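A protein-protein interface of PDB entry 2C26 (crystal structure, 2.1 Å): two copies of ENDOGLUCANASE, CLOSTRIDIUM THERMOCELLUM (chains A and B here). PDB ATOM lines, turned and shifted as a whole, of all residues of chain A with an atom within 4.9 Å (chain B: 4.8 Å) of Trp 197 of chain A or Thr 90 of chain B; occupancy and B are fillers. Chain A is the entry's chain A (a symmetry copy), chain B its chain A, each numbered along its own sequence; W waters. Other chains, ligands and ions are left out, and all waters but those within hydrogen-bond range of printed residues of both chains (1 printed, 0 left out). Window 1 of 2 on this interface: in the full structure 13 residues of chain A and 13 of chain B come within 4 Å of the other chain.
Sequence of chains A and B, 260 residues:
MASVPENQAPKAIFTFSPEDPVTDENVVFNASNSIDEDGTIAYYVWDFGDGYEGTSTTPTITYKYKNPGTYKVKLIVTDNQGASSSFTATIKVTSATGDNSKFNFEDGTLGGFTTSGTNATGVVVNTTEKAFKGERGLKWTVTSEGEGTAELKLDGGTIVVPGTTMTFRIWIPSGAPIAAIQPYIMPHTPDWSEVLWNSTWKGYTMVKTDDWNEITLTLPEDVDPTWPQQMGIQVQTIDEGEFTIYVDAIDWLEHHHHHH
The backbone NH of Trp 197 of chain A lies within hydrogen-bond range of the backbone carbonyl oxygen of Thr 88 of chain B (2.6 Å).
The backbone NH (N) of Thr 88 of chain B lies within hydrogen-bond range of the backbone carbonyl oxygen (O) of Val 195 of chain A (2.9 Å).
OG of Ser 199 of chain A lies within hydrogen-bond range of NE1 of Trp 197 of chain A (2.9 Å).
Among the printed residues, pairs that only touch across the chains: Val 195 of chain A with Phe 87 of chain B, Leu 196 of chain A with Thr 88 of chain B, Trp 197 of chain A with Phe 87 of chain B, Trp 197 of chain A with Ala 89 of chain B and Trp 197 of chain A with Thr 90 of chain B.
Of the printed residues of chain B, Val 195 of chain A touches Phe 87 (3.4 Å) and Thr 88 (2.9 Å).
Printed residues of chain B within 4 Å of Leu 196 of chain A: Thr 88.
Trp 197 of chain A touches just these residues of chain B: Phe 87 (3.5 Å), Thr 88 (2.6 Å), Ala 89 (3.6 Å) and Thr 90 (3.7 Å).
Printed residues of chain A within 4 Å of Phe 87 of chain B: Val 195 (3.4 Å) and Trp 197 (3.5 Å).
Of the printed residues of chain A, Thr 88 of chain B touches Val 195, Leu 196 and Trp 197.
Of the printed residues of chain A, Ala 89 of chain B touches Trp 197.
Of chain A, only Trp 197 (3.7 Å) comes within 4 Å of Thr 90 of chain B.
The nearest printed residue of chain B that does not touch Trp 197 of chain A is Phe 16 of chain B (6.4 Å).
The nearest residue of chain A that does not touch Thr 90 of chain B is Asn 198 of chain A (4.2 Å).
The nearest printed residue of chain B that does not touch Val 195 of chain A is Ala 89 of chain B (5.7 Å).
Hydrophobic or aromatic side chains of chain B within 4 Å of the printed part of chain A: Phe 87.
Of the 10 printed residues of chain A, 3 touch a printed residue of chain B.
No position is printed for both chains.
Water W1 bridges the side-chain hydroxyl (OG1) of Thr 88 of chain B (2.8 Å) and the backbone carbonyl oxygen (O) of Val 195 of chain A (2.9 Å).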
ATOM      1  N   GLN A 182       4.378 -34.190  -3.238  1.00  0.00           N
ATOM      2  CA  GLN A 182       5.138 -33.610  -4.346  1.00  0.00           C
ATOM      3  C   GLN A 182       6.565 -33.218  -3.989  1.00  0.00           C
ATOM      4  O   GLN A 182       6.788 -32.396  -3.098  1.00  0.00           O
ATOM      5  CB  GLN A 182       4.405 -32.404  -4.943  1.00  0.00           C
ATOM      6  CG  GLN A 182       4.096 -31.258  -3.983  1.00  0.00           C
ATOM      7  CD  GLN A 182       3.272 -30.177  -4.649  1.00  0.00           C
ATOM      8  OE1 GLN A 182       3.126 -30.160  -5.872  1.00  0.00           O
ATOM      9  NE2 GLN A 182       2.724 -29.269  -3.853  1.00  0.00           N
ATOM     10  N   TYR A 184       9.661 -30.910  -4.781  1.00  0.00           N
ATOM     11  CA  TYR A 184       9.688 -29.561  -5.314  1.00  0.00           C
ATOM     12  C   TYR A 184      11.093 -28.986  -5.370  1.00  0.00           C
ATOM     13  O   TYR A 184      12.014 -29.452  -4.693  1.00  0.00           O
ATOM     14  CB  TYR A 184       8.726 -28.629  -4.550  1.00  0.00           C
ATOM     15  CG  TYR A 184       9.138 -28.329  -3.115  1.00  0.00           C
ATOM     16  CD1 TYR A 184       9.984 -27.249  -2.813  1.00  0.00           C
ATOM     17  CD2 TYR A 184       8.670 -29.113  -2.068  1.00  0.00           C
ATOM     18  CE1 TYR A 184      10.355 -26.972  -1.495  1.00  0.00           C
ATOM     19  CE2 TYR A 184       9.034 -28.852  -0.753  1.00  0.00           C
ATOM     20  CZ  TYR A 184       9.873 -27.791  -0.472  1.00  0.00           C
ATOM     21  OH  TYR A 184      10.210 -27.554   0.843  1.00  0.00           O
ATOM     22  N   ILE A 185      11.254 -27.986  -6.225  1.00  0.00           N
ATOM     23  CA  ILE A 185      12.445 -27.156  -6.218  1.00  0.00           C
ATOM     24  C   ILE A 185      11.989 -25.700  -6.288  1.00  0.00           C
ATOM     25  O   ILE A 185      11.163 -25.334  -7.116  1.00  0.00           O
ATOM     26  CB  ILE A 185      13.473 -27.539  -7.319  1.00  0.00           C
ATOM     27  CG1 ILE A 185      14.731 -26.664  -7.208  1.00  0.00           C
ATOM     28  CG2 ILE A 185      12.878 -27.441  -8.734  1.00  0.00           C
ATOM     29  CD1 ILE A 185      15.831 -27.260  -6.368  1.00  0.00           C
ATOM     30  N   MET A 186      12.499 -24.891  -5.368  1.00  0.00           N
ATOM     31  CA  MET A 186      12.035 -23.518  -5.198  1.00  0.00           C
ATOM     32  C   MET A 186      13.216 -22.518  -5.155  1.00  0.00           C
ATOM     33  O   MET A 186      13.722 -22.184  -4.065  1.00  0.00           O
ATOM     34  CB  MET A 186      11.133 -23.412  -3.952  1.00  0.00           C
ATOM     35  CG  MET A 186      10.569 -22.005  -3.647  1.00  0.00           C
ATOM     36  SD  MET A 186       9.412 -22.044  -2.256  1.00  0.00           S
ATOM     37  CE  MET A 186      10.486 -22.522  -0.905  1.00  0.00           C
ATOM     38  N   VAL A 195       9.942 -15.649  -5.694  1.00  0.00           N
ATOM     39  CA  VAL A 195      10.013 -17.091  -5.518  1.00  0.00           C
ATOM     40  C   VAL A 195       9.507 -17.803  -6.780  1.00  0.00           C
ATOM     41  O   VAL A 195       8.503 -17.390  -7.365  1.00  0.00           O
ATOM     42  CB  VAL A 195       9.177 -17.530  -4.273  1.00  0.00           C
ATOM     43  CG1 VAL A 195       9.087 -19.029  -4.174  1.00  0.00           C
ATOM     44  CG2 VAL A 195       9.776 -16.946  -2.971  1.00  0.00           C
ATOM     45  N   LEU A 196      10.220 -18.850  -7.209  1.00  0.00           N
ATOM     46  CA  LEU A 196       9.796 -19.713  -8.313  1.00  0.00           C
ATOM     47  C   LEU A 196       9.477 -21.089  -7.763  1.00  0.00           C
ATOM     48  O   LEU A 196      10.193 -21.612  -6.909  1.00  0.00           O
ATOM     49  CB  LEU A 196      10.873 -19.839  -9.394  1.00  0.00           C
ATOM     50  CG  LEU A 196      11.567 -18.567  -9.904  1.00  0.00           C
ATOM     51  CD1 LEU A 196      12.676 -18.949 -10.903  1.00  0.00           C
ATOM     52  CD2 LEU A 196      10.579 -17.577 -10.532  1.00  0.00           C
ATOM     53  N   TRP A 197       8.393 -21.672  -8.249  1.00  0.00           N
ATOM     54  CA  TRP A 197       7.939 -22.942  -7.745  1.00  0.00           C
ATOM     55  C   TRP A 197       7.895 -23.957  -8.869  1.00  0.00           C
ATOM     56  O   TRP A 197       7.271 -23.733  -9.907  1.00  0.00           O
ATOM     57  CB  TRP A 197       6.560 -22.814  -7.080  1.00  0.00           C
ATOM     58  CG  TRP A 197       5.992 -24.130  -6.595  1.00  0.00           C
ATOM     59  CD1 TRP A 197       5.142 -24.966  -7.274  1.00  0.00           C
ATOM     60  CD2 TRP A 197       6.229 -24.748  -5.321  1.00  0.00           C
ATOM     61  NE1 TRP A 197       4.845 -26.067  -6.502  1.00  0.00           N
ATOM     62  CE2 TRP A 197       5.495 -25.959  -5.301  1.00  0.00           C
ATOM     63  CE3 TRP A 197       6.994 -24.397  -4.197  1.00  0.00           C
ATOM     64  CZ2 TRP A 197       5.494 -26.821  -4.192  1.00  0.00           C
ATOM     65  CZ3 TRP A 197       7.009 -25.266  -3.097  1.00  0.00           C
ATOM     66  CH2 TRP A 197       6.249 -26.455  -3.101  1.00  0.00           C
ATOM     67  N   ASN A 198       8.565 -25.079  -8.634  1.00  0.00           N
ATOM     68  CA  ASN A 198       8.545 -26.215  -9.537  1.00  0.00           C
ATOM     69  C   ASN A 198       8.240 -27.462  -8.708  1.00  0.00           C
ATOM     70  O   ASN A 198       8.915 -27.703  -7.712  1.00  0.00           O
ATOM     71  CB  ASN A 198       9.911 -26.350 -10.212  1.00  0.00           C
ATOM     72  CG  ASN A 198      10.263 -25.147 -11.056  1.00  0.00           C
ATOM     73  OD1 ASN A 198       9.784 -25.016 -12.178  1.00  0.00           O
ATOM     74  ND2 ASN A 198      11.103 -24.251 -10.519  1.00  0.00           N
ATOM     75  N   SER A 199       7.208 -28.221  -9.088  1.00  0.00           N
ATOM     76  CA  SER A 199       6.867 -29.471  -8.383  1.00  0.00           C
ATOM     77  C   SER A 199       6.262 -30.556  -9.293  1.00  0.00           C
ATOM     78  O   SER A 199       5.709 -30.252 -10.353  1.00  0.00           O
ATOM     79  CB  SER A 199       5.941 -29.204  -7.188  1.00  0.00           C
ATOM     80  OG  SER A 199       4.644 -28.776  -7.595  1.00  0.00           O
ATOM     81  N   GLN A 234       6.896 -31.996  -0.232  1.00  0.00           N
ATOM     82  CA  GLN A 234       5.739 -31.472   0.485  1.00  0.00           C
ATOM     83  C   GLN A 234       4.587 -32.478   0.492  1.00  0.00           C
ATOM     84  O   GLN A 234       4.221 -33.026  -0.550  1.00  0.00           O
ATOM     85  CB  GLN A 234       5.287 -30.137  -0.127  1.00  0.00           C
ATOM     86  CG  GLN A 234       4.038 -29.547   0.496  1.00  0.00           C
ATOM     87  CD  GLN A 234       3.608 -28.261  -0.184  1.00  0.00           C
ATOM     88  OE1 GLN A 234       3.054 -28.285  -1.280  1.00  0.00           O
ATOM     89  NE2 GLN A 234       3.878 -27.126   0.460  1.00  0.00           N
ATOM     90  N   PHE B  16      -3.395 -23.763  -7.404  1.00  0.00           N
ATOM     91  CA  PHE B  16      -4.415 -23.800  -8.449  1.00  0.00           C
ATOM     92  C   PHE B  16      -5.090 -25.175  -8.533  1.00  0.00           C
ATOM     93  O   PHE B  16      -4.589 -26.163  -7.978  1.00  0.00           O
ATOM     94  CB  PHE B  16      -3.853 -23.345  -9.809  1.00  0.00           C
ATOM     95  CG  PHE B  16      -2.706 -24.186 -10.314  1.00  0.00           C
ATOM     96  CD1 PHE B  16      -2.945 -25.368 -11.000  1.00  0.00           C
ATOM     97  CD2 PHE B  16      -1.387 -23.773 -10.124  1.00  0.00           C
ATOM     98  CE1 PHE B  16      -1.893 -26.153 -11.471  1.00  0.00           C
ATOM     99  CE2 PHE B  16      -0.323 -24.550 -10.592  1.00  0.00           C
ATOM    100  CZ  PHE B  16      -0.577 -25.742 -11.267  1.00  0.00           C
ATOM    101  N   THR B  70       3.074 -25.562 -21.462  1.00  0.00           N
ATOM    102  CA  THR B  70       3.494 -25.335 -20.096  1.00  0.00           C
ATOM    103  C   THR B  70       3.608 -23.814 -19.933  1.00  0.00           C
ATOM    104  O   THR B  70       4.371 -23.170 -20.653  1.00  0.00           O
ATOM    105  CB  THR B  70       4.842 -26.058 -19.816  1.00  0.00           C
ATOM    106  OG1 THR B  70       4.645 -27.480 -19.860  1.00  0.00           O
ATOM    107  CG2 THR B  70       5.397 -25.685 -18.461  1.00  0.00           C
ATOM    108  N   TYR B  71       2.828 -23.256 -19.006  1.00  0.00           N
ATOM    109  CA  TYR B  71       2.761 -21.807 -18.780  1.00  0.00           C
ATOM    110  C   TYR B  71       3.362 -21.426 -17.422  1.00  0.00           C
ATOM    111  O   TYR B  71       3.180 -22.142 -16.437  1.00  0.00           O
ATOM    112  CB  TYR B  71       1.311 -21.307 -18.874  1.00  0.00           C
ATOM    113  CG  TYR B  71       0.658 -21.570 -20.221  1.00  0.00           C
ATOM    114  CD1 TYR B  71       0.741 -20.629 -21.255  1.00  0.00           C
ATOM    115  CD2 TYR B  71      -0.009 -22.783 -20.480  1.00  0.00           C
ATOM    116  CE1 TYR B  71       0.168 -20.878 -22.498  1.00  0.00           C
ATOM    117  CE2 TYR B  71      -0.600 -23.030 -21.724  1.00  0.00           C
ATOM    118  CZ  TYR B  71      -0.502 -22.066 -22.726  1.00  0.00           C
ATOM    119  OH  TYR B  71      -1.072 -22.300 -23.960  1.00  0.00           O
ATOM    120  N   LYS B  72       4.094 -20.316 -17.381  1.00  0.00           N
ATOM    121  CA  LYS B  72       4.545 -19.753 -16.111  1.00  0.00           C
ATOM    122  C   LYS B  72       3.474 -18.820 -15.607  1.00  0.00           C
ATOM    123  O   LYS B  72       3.160 -17.825 -16.272  1.00  0.00           O
ATOM    124  CB  LYS B  72       5.852 -18.967 -16.284  1.00  0.00           C
ATOM    125  CG  LYS B  72       7.027 -19.818 -16.668  1.00  0.00           C
ATOM    126  CD  LYS B  72       8.193 -18.999 -17.240  1.00  0.00           C
ATOM    127  CE  LYS B  72       8.384 -17.659 -16.520  1.00  0.00           C
ATOM    128  NZ  LYS B  72       8.768 -17.789 -15.063  1.00  0.00           N
ATOM    129  N   PHE B  87       5.355 -14.674  -6.690  1.00  0.00           N
ATOM    130  CA  PHE B  87       5.400 -16.122  -6.608  1.00  0.00           C
ATOM    131  C   PHE B  87       5.027 -16.635  -7.981  1.00  0.00           C
ATOM    132  O   PHE B  87       3.979 -16.269  -8.514  1.00  0.00           O
ATOM    133  CB  PHE B  87       4.406 -16.630  -5.556  1.00  0.00           C
ATOM    134  CG  PHE B  87       4.486 -18.113  -5.314  1.00  0.00           C
ATOM    135  CD1 PHE B  87       3.694 -18.997  -6.041  1.00  0.00           C
ATOM    136  CD2 PHE B  87       5.368 -18.630  -4.365  1.00  0.00           C
ATOM    137  CE1 PHE B  87       3.772 -20.376  -5.807  1.00  0.00           C
ATOM    138  CE2 PHE B  87       5.455 -19.984  -4.135  1.00  0.00           C
ATOM    139  CZ  PHE B  87       4.654 -20.867  -4.849  1.00  0.00           C
ATOM    140  N   THR B  88       5.883 -17.462  -8.562  1.00  0.00           N
ATOM    141  CA  THR B  88       5.654 -17.976  -9.902  1.00  0.00           C
ATOM    142  C   THR B  88       5.614 -19.500  -9.859  1.00  0.00           C
ATOM    143  O   THR B  88       6.537 -20.130  -9.328  1.00  0.00           O
ATOM    144  CB  THR B  88       6.758 -17.495 -10.897  1.00  0.00           C
ATOM    145  OG1 THR B  88       6.813 -16.068 -10.906  1.00  0.00           O
ATOM    146  CG2 THR B  88       6.521 -18.005 -12.318  1.00  0.00           C
ATOM    147  N   ALA B  89       4.534 -20.083 -10.385  1.00  0.00           N
ATOM    148  CA  ALA B  89       4.425 -21.541 -10.519  1.00  0.00           C
ATOM    149  C   ALA B  89       4.194 -21.919 -11.972  1.00  0.00           C
ATOM    150  O   ALA B  89       3.717 -21.101 -12.755  1.00  0.00           O
ATOM    151  CB  ALA B  89       3.300 -22.095  -9.638  1.00  0.00           C
ATOM    152  N   THR B  90       4.526 -23.157 -12.325  1.00  0.00           N
ATOM    153  CA  THR B  90       4.326 -23.672 -13.679  1.00  0.00           C
ATOM    154  C   THR B  90       3.043 -24.505 -13.756  1.00  0.00           C
ATOM    155  O   THR B  90       2.732 -25.258 -12.834  1.00  0.00           O
ATOM    156  CB  THR B  90       5.562 -24.493 -14.123  1.00  0.00           C
ATOM    157  OG1 THR B  90       6.603 -23.593 -14.532  1.00  0.00           O
ATOM    158  CG2 THR B  90       5.237 -25.441 -15.286  1.00  0.00           C
ATOM    159  N   ILE B  91       2.297 -24.356 -14.848  1.00  0.00           N
ATOM    160  CA  ILE B  91       1.070 -25.118 -15.061  1.00  0.00           C
ATOM    161  C   ILE B  91       1.101 -25.763 -16.446  1.00  0.00           C
ATOM    162  O   ILE B  91       1.433 -25.115 -17.433  1.00  0.00           O
ATOM    163  CB  ILE B  91      -0.234 -24.251 -14.812  1.00  0.00           C
ATOM    164  CG1 ILE B  91      -1.495 -25.129 -14.887  1.00  0.00           C
ATOM    165  CG2 ILE B  91      -0.339 -23.080 -15.777  1.00  0.00           C
ATOM    166  CD1 ILE B  91      -2.809 -24.410 -14.531  1.00  0.00           C
ATOM    167  N   LYS B  92       0.780 -27.052 -16.508  1.00  0.00           N
ATOM    168  CA  LYS B  92       0.789 -27.777 -17.767  1.00  0.00           C
ATOM    169  C   LYS B  92      -0.624 -27.969 -18.257  1.00  0.00           C
ATOM    170  O   LYS B  92      -1.489 -28.436 -17.521  1.00  0.00           O
ATOM    171  CB  LYS B  92       1.510 -29.136 -17.635  1.00  0.00           C
ATOM    172  CG  LYS B  92       1.707 -29.859 -18.968  1.00  0.00           C
ATOM    173  CD  LYS B  92       2.688 -31.032 -18.848  1.00  0.00           C
ATOM    174  CE  LYS B  92       3.015 -31.612 -20.221  1.00  0.00           C
ATOM    175  NZ  LYS B  92       3.746 -32.928 -20.152  1.00  0.00           N
HETATM  176  O   HOH W   1       8.178 -14.870  -8.791  1.00  0.00           O
